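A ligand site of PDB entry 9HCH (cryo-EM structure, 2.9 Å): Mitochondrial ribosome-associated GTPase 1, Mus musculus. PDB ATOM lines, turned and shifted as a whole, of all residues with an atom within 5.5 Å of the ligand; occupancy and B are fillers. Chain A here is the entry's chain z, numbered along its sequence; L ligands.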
ATOM      1  N   ASN A  82      -8.893  26.709   2.546  1.00  0.00           N
ATOM      2  CA  ASN A  82      -8.701  25.818   3.673  1.00  0.00           C
ATOM      3  C   ASN A  82      -8.759  24.358   3.218  1.00  0.00           C
ATOM      4  O   ASN A  82      -9.052  24.050   2.061  1.00  0.00           O
ATOM      5  CB  ASN A  82      -9.760  26.094   4.742  1.00  0.00           C
ATOM      6  CG  ASN A  82      -9.402  25.481   6.084  1.00  0.00           C
ATOM      7  OD1 ASN A  82      -8.226  25.346   6.423  1.00  0.00           O
ATOM      8  ND2 ASN A  82     -10.413  25.094   6.844  1.00  0.00           N
ATOM      9  N   LYS A  83      -8.462  23.457   4.150  1.00  0.00           N
ATOM     10  CA  LYS A  83      -8.541  22.019   3.902  1.00  0.00           C
ATOM     11  C   LYS A  83      -7.619  21.599   2.764  1.00  0.00           C
ATOM     12  O   LYS A  83      -7.968  20.790   1.910  1.00  0.00           O
ATOM     13  CB  LYS A  83      -9.982  21.587   3.605  1.00  0.00           C
ATOM     14  CG  LYS A  83     -10.923  21.739   4.786  1.00  0.00           C
ATOM     15  CD  LYS A  83     -12.330  21.281   4.442  1.00  0.00           C
ATOM     16  CE  LYS A  83     -13.287  21.485   5.594  1.00  0.00           C
ATOM     17  NZ  LYS A  83     -14.703  21.294   5.192  1.00  0.00           N
ATOM     18  N   MET A  84      -6.406  22.167   2.745  1.00  0.00           N
ATOM     19  CA  MET A  84      -5.439  21.829   1.713  1.00  0.00           C
ATOM     20  C   MET A  84      -4.841  20.442   1.906  1.00  0.00           C
ATOM     21  O   MET A  84      -4.375  19.841   0.930  1.00  0.00           O
ATOM     22  CB  MET A  84      -4.319  22.876   1.693  1.00  0.00           C
ATOM     23  CG  MET A  84      -3.407  22.828   2.914  1.00  0.00           C
ATOM     24  SD  MET A  84      -2.221  24.193   2.951  1.00  0.00           S
ATOM     25  CE  MET A  84      -1.123  23.734   1.618  1.00  0.00           C
ATOM     26  N   ASP A  85      -4.848  19.910   3.140  1.00  0.00           N
ATOM     27  CA  ASP A  85      -4.211  18.632   3.385  1.00  0.00           C
ATOM     28  C   ASP A  85      -4.901  17.494   2.643  1.00  0.00           C
ATOM     29  O   ASP A  85      -4.244  16.661   2.012  1.00  0.00           O
ATOM     30  CB  ASP A  85      -4.174  18.345   4.885  1.00  0.00           C
ATOM     31  CG  ASP A  85      -5.550  18.394   5.517  1.00  0.00           C
ATOM     32  OD1 ASP A  85      -6.423  19.113   4.980  1.00  0.00           O
ATOM     33  OD2 ASP A  85      -5.761  17.715   6.540  1.00  0.00           O
ATOM     34  N   LEU A  86      -6.235  17.458   2.682  1.00  0.00           N
ATOM     35  CA  LEU A  86      -6.992  16.391   2.018  1.00  0.00           C
ATOM     36  C   LEU A  86      -7.339  16.810   0.586  1.00  0.00           C
ATOM     37  O   LEU A  86      -8.486  16.816   0.144  1.00  0.00           O
ATOM     38  CB  LEU A  86      -8.230  16.033   2.829  1.00  0.00           C
ATOM     39  CG  LEU A  86      -9.449  16.965   2.898  1.00  0.00           C
ATOM     40  CD1 LEU A  86     -10.655  16.205   3.430  1.00  0.00           C
ATOM     41  CD2 LEU A  86      -9.139  18.161   3.761  1.00  0.00           C
ATOM     42  N   THR A 110      -4.341  26.955   3.235  1.00  0.00           N
ATOM     43  CA  THR A 110      -4.235  26.817   4.682  1.00  0.00           C
ATOM     44  C   THR A 110      -4.825  25.489   5.135  1.00  0.00           C
ATOM     45  O   THR A 110      -5.813  25.006   4.572  1.00  0.00           O
ATOM     46  CB  THR A 110      -4.961  27.960   5.410  1.00  0.00           C
ATOM     47  OG1 THR A 110      -6.374  27.790   5.262  1.00  0.00           O
ATOM     48  CG2 THR A 110      -4.552  29.300   4.839  1.00  0.00           C
ATOM     49  N   ASN A 111      -4.210  24.907   6.165  1.00  0.00           N
ATOM     50  CA  ASN A 111      -4.762  23.771   6.889  1.00  0.00           C
ATOM     51  C   ASN A 111      -4.960  24.195   8.340  1.00  0.00           C
ATOM     52  O   ASN A 111      -3.999  24.632   8.988  1.00  0.00           O
ATOM     53  CB  ASN A 111      -3.834  22.557   6.802  1.00  0.00           C
ATOM     54  CG  ASN A 111      -4.383  21.348   7.528  1.00  0.00           C
ATOM     55  OD1 ASN A 111      -5.468  21.406   8.116  1.00  0.00           O
ATOM     56  ND2 ASN A 111      -3.636  20.250   7.504  1.00  0.00           N
ATOM     57  N   CYS A 112      -6.191  24.067   8.838  1.00  0.00           N
ATOM     58  CA  CYS A 112      -6.510  24.569  10.171  1.00  0.00           C
ATOM     59  C   CYS A 112      -6.391  23.513  11.259  1.00  0.00           C
ATOM     60  O   CYS A 112      -6.168  23.873  12.425  1.00  0.00           O
ATOM     61  CB  CYS A 112      -7.924  25.145  10.184  1.00  0.00           C
ATOM     62  SG  CYS A 112      -8.056  26.785   9.440  1.00  0.00           S
ATOM     63  N   VAL A 113      -6.544  22.228  10.931  1.00  0.00           N
ATOM     64  CA  VAL A 113      -6.379  21.197  11.959  1.00  0.00           C
ATOM     65  C   VAL A 113      -4.916  21.067  12.358  1.00  0.00           C
ATOM     66  O   VAL A 113      -4.599  20.834  13.534  1.00  0.00           O
ATOM     67  CB  VAL A 113      -6.961  19.848  11.476  1.00  0.00           C
ATOM     68  CG1 VAL A 113      -8.478  19.892  11.491  1.00  0.00           C
ATOM     69  CG2 VAL A 113      -6.432  19.477  10.104  1.00  0.00           C
ATOM     70  N   VAL A 150     -18.905  29.726   2.173  1.00  0.00           N
ATOM     71  CA  VAL A 150     -19.947  28.703   2.141  1.00  0.00           C
ATOM     72  C   VAL A 150     -19.815  27.872   3.410  1.00  0.00           C
ATOM     73  O   VAL A 150     -18.717  27.771   3.967  1.00  0.00           O
ATOM     74  CB  VAL A 150     -19.834  27.826   0.877  1.00  0.00           C
ATOM     75  CG1 VAL A 150     -19.963  28.685  -0.371  1.00  0.00           C
ATOM     76  CG2 VAL A 150     -18.535  27.044   0.866  1.00  0.00           C
ATOM     77  N   PRO A 151     -20.888  27.257   3.903  1.00  0.00           N
ATOM     78  CA  PRO A 151     -20.797  26.548   5.187  1.00  0.00           C
ATOM     79  C   PRO A 151     -19.864  25.353   5.123  1.00  0.00           C
ATOM     80  O   PRO A 151     -19.683  24.741   4.066  1.00  0.00           O
ATOM     81  CB  PRO A 151     -22.252  26.118   5.464  1.00  0.00           C
ATOM     82  CG  PRO A 151     -23.098  26.852   4.474  1.00  0.00           C
ATOM     83  CD  PRO A 151     -22.223  27.124   3.304  1.00  0.00           C
ATOM     84  N   ASN A 152     -19.262  25.035   6.266  1.00  0.00           N
ATOM     85  CA  ASN A 152     -18.409  23.860   6.410  1.00  0.00           C
ATOM     86  C   ASN A 152     -17.136  23.978   5.587  1.00  0.00           C
ATOM     87  O   ASN A 152     -16.723  23.027   4.916  1.00  0.00           O
ATOM     88  CB  ASN A 152     -19.171  22.579   6.044  1.00  0.00           C
ATOM     89  CG  ASN A 152     -18.578  21.341   6.688  1.00  0.00           C
ATOM     90  OD1 ASN A 152     -17.992  21.407   7.774  1.00  0.00           O
ATOM     91  ND2 ASN A 152     -18.729  20.205   6.024  1.00  0.00           N
ATOM     92  N   VAL A 153     -16.498  25.150   5.630  1.00  0.00           N
ATOM     93  CA  VAL A 153     -15.198  25.362   5.006  1.00  0.00           C
ATOM     94  C   VAL A 153     -14.101  25.625   6.017  1.00  0.00           C
ATOM     95  O   VAL A 153     -12.934  25.729   5.637  1.00  0.00           O
ATOM     96  CB  VAL A 153     -15.251  26.513   3.977  1.00  0.00           C
ATOM     97  CG1 VAL A 153     -16.063  26.108   2.768  1.00  0.00           C
ATOM     98  CG2 VAL A 153     -15.785  27.787   4.608  1.00  0.00           C
ATOM     99  N   GLY A 154     -14.449  25.724   7.304  1.00  0.00           N
ATOM    100  CA  GLY A 154     -13.458  26.007   8.321  1.00  0.00           C
ATOM    101  C   GLY A 154     -13.314  27.478   8.672  1.00  0.00           C
ATOM    102  O   GLY A 154     -12.240  27.884   9.122  1.00  0.00           O
ATOM    103  N   LYS A 155     -14.355  28.276   8.469  1.00  0.00           N
ATOM    104  CA  LYS A 155     -14.300  29.671   8.885  1.00  0.00           C
ATOM    105  C   LYS A 155     -14.101  29.773  10.393  1.00  0.00           C
ATOM    106  O   LYS A 155     -13.234  30.513  10.870  1.00  0.00           O
ATOM    107  CB  LYS A 155     -15.573  30.410   8.464  1.00  0.00           C
ATOM    108  CG  LYS A 155     -15.960  30.206   7.002  1.00  0.00           C
ATOM    109  CD  LYS A 155     -17.113  31.108   6.578  1.00  0.00           C
ATOM    110  CE  LYS A 155     -18.310  31.017   7.510  1.00  0.00           C
ATOM    111  NZ  LYS A 155     -18.852  29.635   7.591  1.00  0.00           N
ATOM    112  N   SER A 156     -14.916  29.037  11.159  1.00  0.00           N
ATOM    113  CA  SER A 156     -14.772  29.055  12.603  1.00  0.00           C
ATOM    114  C   SER A 156     -13.460  28.429  13.052  1.00  0.00           C
ATOM    115  O   SER A 156     -12.880  28.852  14.054  1.00  0.00           O
ATOM    116  CB  SER A 156     -15.953  28.322  13.250  1.00  0.00           C
ATOM    117  OG  SER A 156     -17.184  28.755  12.691  1.00  0.00           O
ATOM    118  N   SER A 157     -12.982  27.412  12.324  1.00  0.00           N
ATOM    119  CA  SER A 157     -11.686  26.819  12.642  1.00  0.00           C
ATOM    120  C   SER A 157     -10.563  27.839  12.452  1.00  0.00           C
ATOM    121  O   SER A 157      -9.671  27.957  13.298  1.00  0.00           O
ATOM    122  CB  SER A 157     -11.449  25.592  11.773  1.00  0.00           C
ATOM    123  OG  SER A 157     -12.404  24.580  12.046  1.00  0.00           O
ATOM    124  N   LEU A 158     -10.587  28.570  11.343  1.00  0.00           N
ATOM    125  CA  LEU A 158      -9.565  29.570  11.087  1.00  0.00           C
ATOM    126  C   LEU A 158      -9.446  30.543  12.248  1.00  0.00           C
ATOM    127  O   LEU A 158      -8.340  30.932  12.650  1.00  0.00           O
ATOM    128  CB  LEU A 158      -9.876  30.321   9.786  1.00  0.00           C
ATOM    129  CG  LEU A 158      -8.850  31.338   9.284  1.00  0.00           C
ATOM    130  CD1 LEU A 158      -8.945  31.471   7.774  1.00  0.00           C
ATOM    131  CD2 LEU A 158      -9.042  32.697   9.948  1.00  0.00           C
ATOM    132  N   ARG A 174     -17.329  27.908  18.407  1.00  0.00           N
ATOM    133  CA  ARG A 174     -17.692  26.505  18.385  1.00  0.00           C
ATOM    134  C   ARG A 174     -17.435  25.913  17.007  1.00  0.00           C
ATOM    135  O   ARG A 174     -17.830  26.493  15.988  1.00  0.00           O
ATOM    136  CB  ARG A 174     -19.169  26.335  18.772  1.00  0.00           C
ATOM    137  CG  ARG A 174     -19.658  24.898  18.764  1.00  0.00           C
ATOM    138  CD  ARG A 174     -21.121  24.811  19.134  1.00  0.00           C
ATOM    139  NE  ARG A 174     -21.346  24.947  20.568  1.00  0.00           N
ATOM    140  CZ  ARG A 174     -22.531  25.001  21.145  1.00  0.00           C
ATOM    141  NH1 ARG A 174     -23.649  24.948  20.438  1.00  0.00           N
ATOM    142  NH2 ARG A 174     -22.607  25.108  22.472  1.00  0.00           N
ATOM    143  N   VAL A 175     -16.754  24.778  16.975  1.00  0.00           N
ATOM    144  CA  VAL A 175     -16.342  24.104  15.746  1.00  0.00           C
ATOM    145  C   VAL A 175     -17.027  22.749  15.694  1.00  0.00           C
ATOM    146  O   VAL A 175     -17.024  22.013  16.687  1.00  0.00           O
ATOM    147  CB  VAL A 175     -14.818  23.968  15.668  1.00  0.00           C
ATOM    148  CG1 VAL A 175     -14.412  22.868  14.703  1.00  0.00           C
ATOM    149  CG2 VAL A 175     -14.196  25.291  15.247  1.00  0.00           C
ATOM    150  N   GLY A 176     -17.598  22.413  14.544  1.00  0.00           N
ATOM    151  CA  GLY A 176     -18.367  21.194  14.398  1.00  0.00           C
ATOM    152  C   GLY A 176     -18.092  20.541  13.052  1.00  0.00           C
ATOM    153  O   GLY A 176     -17.568  21.167  12.125  1.00  0.00           O
ATOM    154  N   GLY A 177     -18.469  19.265  12.967  1.00  0.00           N
ATOM    155  CA  GLY A 177     -18.239  18.495  11.765  1.00  0.00           C
ATOM    156  C   GLY A 177     -19.422  18.476  10.817  1.00  0.00           C
ATOM    157  O   GLY A 177     -19.505  17.623   9.937  1.00  0.00           O
ATOM    158  N   GLU A 178     -20.333  19.421  10.992  1.00  0.00           N
ATOM    159  CA  GLU A 178     -21.568  19.485  10.222  1.00  0.00           C
ATOM    160  C   GLU A 178     -21.764  20.890   9.676  1.00  0.00           C
ATOM    161  O   GLU A 178     -21.371  21.864  10.331  1.00  0.00           O
ATOM    162  CB  GLU A 178     -22.773  19.100  11.103  1.00  0.00           C
ATOM    163  CG  GLU A 178     -24.085  18.951  10.357  1.00  0.00           C
ATOM    164  CD  GLU A 178     -25.204  18.427  11.240  1.00  0.00           C
ATOM    165  OE1 GLU A 178     -24.964  18.229  12.447  1.00  0.00           O
ATOM    166  OE2 GLU A 178     -26.317  18.217  10.724  1.00  0.00           O
ATOM    167  N   PRO A 179     -22.330  21.030   8.476  1.00  0.00           N
ATOM    168  CA  PRO A 179     -22.553  22.369   7.937  1.00  0.00           C
ATOM    169  C   PRO A 179     -23.641  23.119   8.682  1.00  0.00           C
ATOM    170  O   PRO A 179     -24.693  22.562   9.025  1.00  0.00           O
ATOM    171  CB  PRO A 179     -22.966  22.098   6.483  1.00  0.00           C
ATOM    172  CG  PRO A 179     -23.507  20.708   6.496  1.00  0.00           C
ATOM    173  CD  PRO A 179     -22.655  19.987   7.487  1.00  0.00           C
ATOM    174  N   GLY A 180     -23.381  24.398   8.943  1.00  0.00           N
ATOM    175  CA  GLY A 180     -24.374  25.260   9.562  1.00  0.00           C
ATOM    176  C   GLY A 180     -24.356  25.270  11.074  1.00  0.00           C
ATOM    177  O   GLY A 180     -25.411  25.251  11.704  1.00  0.00           O
ATOM    178  N   ILE A 181     -23.165  25.285  11.666  1.00  0.00           N
ATOM    179  CA  ILE A 181     -23.053  25.324  13.135  1.00  0.00           C
ATOM    180  C   ILE A 181     -23.084  26.750  13.649  1.00  0.00           C
ATOM    181  O   ILE A 181     -23.718  27.030  14.672  1.00  0.00           O
ATOM    182  CB  ILE A 181     -21.782  24.574  13.591  1.00  0.00           C
ATOM    183  CG1 ILE A 181     -20.533  25.223  13.009  1.00  0.00           C
ATOM    184  CG2 ILE A 181     -21.868  23.113  13.191  1.00  0.00           C
ATOM    185  CD1 ILE A 181     -19.260  24.744  13.634  1.00  0.00           C
ATOM    186  N   THR A 182     -22.398  27.675  12.976  1.00  0.00           N
ATOM    187  CA  THR A 182     -22.406  29.081  13.367  1.00  0.00           C
ATOM    188  C   THR A 182     -23.587  29.767  12.692  1.00  0.00           C
ATOM    189  O   THR A 182     -23.700  29.743  11.465  1.00  0.00           O
ATOM    190  CB  THR A 182     -21.064  29.740  13.011  1.00  0.00           C
ATOM    191  OG1 THR A 182     -21.093  31.118  13.393  1.00  0.00           O
ATOM    192  CG2 THR A 182     -20.739  29.609  11.518  1.00  0.00           C
ATOM    193  N   ASP A 201     -16.946  36.637  12.988  1.00  0.00           N
ATOM    194  CA  ASP A 201     -17.385  35.346  12.485  1.00  0.00           C
ATOM    195  C   ASP A 201     -18.803  35.461  11.963  1.00  0.00           C
ATOM    196  O   ASP A 201     -19.668  36.036  12.631  1.00  0.00           O
ATOM    197  CB  ASP A 201     -17.312  34.273  13.583  1.00  0.00           C
ATOM    198  CG  ASP A 201     -17.359  32.869  13.021  1.00  0.00           C
ATOM    199  OD1 ASP A 201     -17.249  32.710  11.781  1.00  0.00           O
ATOM    200  OD2 ASP A 201     -17.503  31.916  13.812  1.00  0.00           O
ATOM    201  N   THR A 202     -19.051  34.909  10.776  1.00  0.00           N
ATOM    202  CA  THR A 202     -20.339  35.001  10.111  1.00  0.00           C
ATOM    203  C   THR A 202     -20.821  33.614   9.715  1.00  0.00           C
ATOM    204  O   THR A 202     -20.001  32.732   9.420  1.00  0.00           O
ATOM    205  CB  THR A 202     -20.254  35.887   8.866  1.00  0.00           C
ATOM    206  OG1 THR A 202     -19.564  35.189   7.825  1.00  0.00           O
ATOM    207  CG2 THR A 202     -19.537  37.192   9.166  1.00  0.00           C
ATOM    208  N   PRO A 203     -22.139  33.403   9.687  1.00  0.00           N
ATOM    209  CA  PRO A 203     -22.651  32.110   9.235  1.00  0.00           C
ATOM    210  C   PRO A 203     -22.352  31.871   7.756  1.00  0.00           C
ATOM    211  O   PRO A 203     -22.299  32.801   6.951  1.00  0.00           O
ATOM    212  CB  PRO A 203     -24.160  32.232   9.476  1.00  0.00           C
ATOM    213  CG  PRO A 203     -24.427  33.693   9.439  1.00  0.00           C
ATOM    214  CD  PRO A 203     -23.222  34.331  10.045  1.00  0.00           C
ATOM    215  N   GLY A 204     -22.142  30.601   7.426  1.00  0.00           N
ATOM    216  CA  GLY A 204     -21.858  30.259   6.048  1.00  0.00           C
ATOM    217  C   GLY A 204     -23.051  30.550   5.150  1.00  0.00           C
ATOM    218  O   GLY A 204     -24.205  30.269   5.495  1.00  0.00           O
ATOM    219  N   SER A 310     -12.880  12.170   5.408  1.00  0.00           N
ATOM    220  CA  SER A 310     -11.723  12.082   6.300  1.00  0.00           C
ATOM    221  C   SER A 310     -10.426  12.189   5.528  1.00  0.00           C
ATOM    222  O   SER A 310      -9.438  12.733   6.048  1.00  0.00           O
ATOM    223  CB  SER A 310     -11.771  10.776   7.086  1.00  0.00           C
ATOM    224  OG  SER A 310     -11.659   9.662   6.220  1.00  0.00           O
HETATM  225  P1  LIG L   1     -20.503  26.745   9.229  1.00  0.00           P
HETATM  226  O1  LIG L   1     -20.920  25.811   8.135  1.00  0.00           O
HETATM  227  O2  LIG L   1     -20.564  28.157   8.714  1.00  0.00           O
HETATM  228  O3  LIG L   1     -21.400  26.592  10.426  1.00  0.00           O
HETATM  229  N1  LIG L   1     -18.998  26.399   9.769  1.00  0.00           N
HETATM  230  P2  LIG L   1     -17.562  26.945   9.241  1.00  0.00           P
HETATM  231  O4  LIG L   1     -17.025  28.010  10.104  1.00  0.00           O
HETATM  232  O5  LIG L   1     -17.619  27.381   7.833  1.00  0.00           O
HETATM  233  O6  LIG L   1     -16.522  25.758   9.424  1.00  0.00           O
HETATM  234  P3  LIG L   1     -15.980  25.016  10.729  1.00  0.00           P
HETATM  235  O7  LIG L   1     -17.107  24.778  11.654  1.00  0.00           O
HETATM  236  O8  LIG L   1     -14.782  25.714  11.216  1.00  0.00           O
HETATM  237  O9  LIG L   1     -15.557  23.584  10.151  1.00  0.00           O
HETATM  238  C1  LIG L   1     -15.079  22.605  11.084  1.00  0.00           C
HETATM  239  C2  LIG L   1     -15.091  21.233  10.456  1.00  0.00           C
HETATM  240  O10 LIG L   1     -14.196  21.225   9.330  1.00  0.00           O
HETATM  241  C3  LIG L   1     -14.596  20.122  11.360  1.00  0.00           C
HETATM  242  O11 LIG L   1     -15.128  18.876  10.937  1.00  0.00           O
HETATM  243  C4  LIG L   1     -13.084  20.211  11.147  1.00  0.00           C
HETATM  244  O12 LIG L   1     -12.376  19.025  11.511  1.00  0.00           O
HETATM  245  C5  LIG L   1     -13.036  20.462   9.643  1.00  0.00           C
HETATM  246  N2  LIG L   1     -11.856  21.214   9.214  1.00  0.00           N
HETATM  247  C6  LIG L   1     -11.621  22.547   9.348  1.00  0.00           C
HETATM  248  N3  LIG L   1     -10.457  22.916   8.854  1.00  0.00           N
HETATM  249  C7  LIG L   1      -9.896  21.743   8.373  1.00  0.00           C
HETATM  250  C8  LIG L   1      -8.646  21.481   7.726  1.00  0.00           C
HETATM  251  O13 LIG L   1      -7.799  22.339   7.473  1.00  0.00           O
HETATM  252  N4  LIG L   1      -8.485  20.203   7.405  1.00  0.00           N
HETATM  253  C9  LIG L   1      -9.389  19.207   7.659  1.00  0.00           C
HETATM  254  N5  LIG L   1      -9.044  17.972   7.273  1.00  0.00           N
HETATM  255  N6  LIG L   1     -10.556  19.409   8.258  1.00  0.00           N
HETATM  256  C10 LIG L   1     -10.747  20.693   8.585  1.00  0.00           C
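Residues that only touch the ligand: Lys 83 (3.6 Å), Leu 86 (3.5 Å), Val 113 (3.5 Å), Pro 151 (3.0 Å), Val 175 (3.7 Å), Gly 176 (3.0 Å), Gly 177 (3.2 Å) and Pro 179 (3.8 Å).
Hydrophobic or aromatic side chains that line the ligand: Leu 86, Val 113, Pro 151, Val 153, Val 175 and Ile 181.
Of the 32 residues printed, 22 come within 4 Å of the ligand.
O of Val 153 lies within hydrogen-bond range of ND2 of Asn 82 (2.9 Å).
The side-chain amide oxygen (OD1) of Asn 111 lies close to the backbone NH (N) of Val 113 (3.1 Å).
The backbone carbonyl oxygen (O) of Asn 152 sits at hydrogen-bond distance from the side-chain amino group (NZ) of Lys 83 (2.7 Å).
The side-chain amide oxygen of Asn 82 lies close to the backbone carbonyl oxygen of Thr 110, 3.1 Å away.
ND2 of Asn 111 sits close to OD2 of Asp 85 (3.4 Å).
OD1 of Asn 82 sits at hydrogen-bond distance from SG of Cys 112, 3.3 Å away.
O of Thr 110 sits at hydrogen-bond distance from N of Lys 83, 3.1 Å away.
The side-chain sulfur (SG) of Cys 112 lies close to the backbone NH (N) of Leu 158, at 3.6 Å.
The side-chain amino group (NZ) of Lys 155 lies within salt-bridge range of an oxygen (O2) of the ligand (2.5 Å).
The side-chain hydroxyl (OG) of Ser 157 lies within hydrogen-bond range of an oxygen (O8) of the ligand, at 2.8 Å.
The backbone NH (N) of Ser 156 sits at hydrogen-bond distance from an oxygen (O4) of the ligand.
An oxygen (O4) of the ligand lies within hydrogen-bond range of the side-chain hydroxyl of Ser 156, at 2.7 Å.
The backbone NH of Gly 180 sits at hydrogen-bond distance from an oxygen (O1) of the ligand, at 3.0 Å.
An oxygen (O13) of the ligand is in hydrogen-bond range of the backbone NH (N) of Cys 112.
ND2 of Asn 82 sits at hydrogen-bond distance from N3 of the ligand (3.0 Å).
The backbone NH (N) of Gly 204 is in hydrogen-bond range of an oxygen (O2) of the ligand (3.2 Å).
N of Thr 182 is in hydrogen-bond range of O3 of the ligand, at 2.9 Å.
N of Val 153 is in hydrogen-bond range of O5 of the ligand (3.3 Å).
The backbone NH of Lys 155 lies within hydrogen-bond range of an oxygen (O4) of the ligand.
An oxygen (O1) of the ligand is in hydrogen-bond range of the backbone NH of Asn 152 (2.6 Å).
The backbone NH (N) of Gly 154 lies within hydrogen-bond range of an oxygen (O6) of the ligand, 3.0 Å away.
OD1 of Asp 85 lies within hydrogen-bond range of N4 of the ligand (3.4 Å).
An oxygen (O3) of the ligand sits at hydrogen-bond distance from the backbone NH (N) of Ile 181.
OD1 of Asn 111 lies close to O13 of the ligand, 2.6 Å away.
N of Ser 157 is in hydrogen-bond range of O8 of the ligand (2.7 Å).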
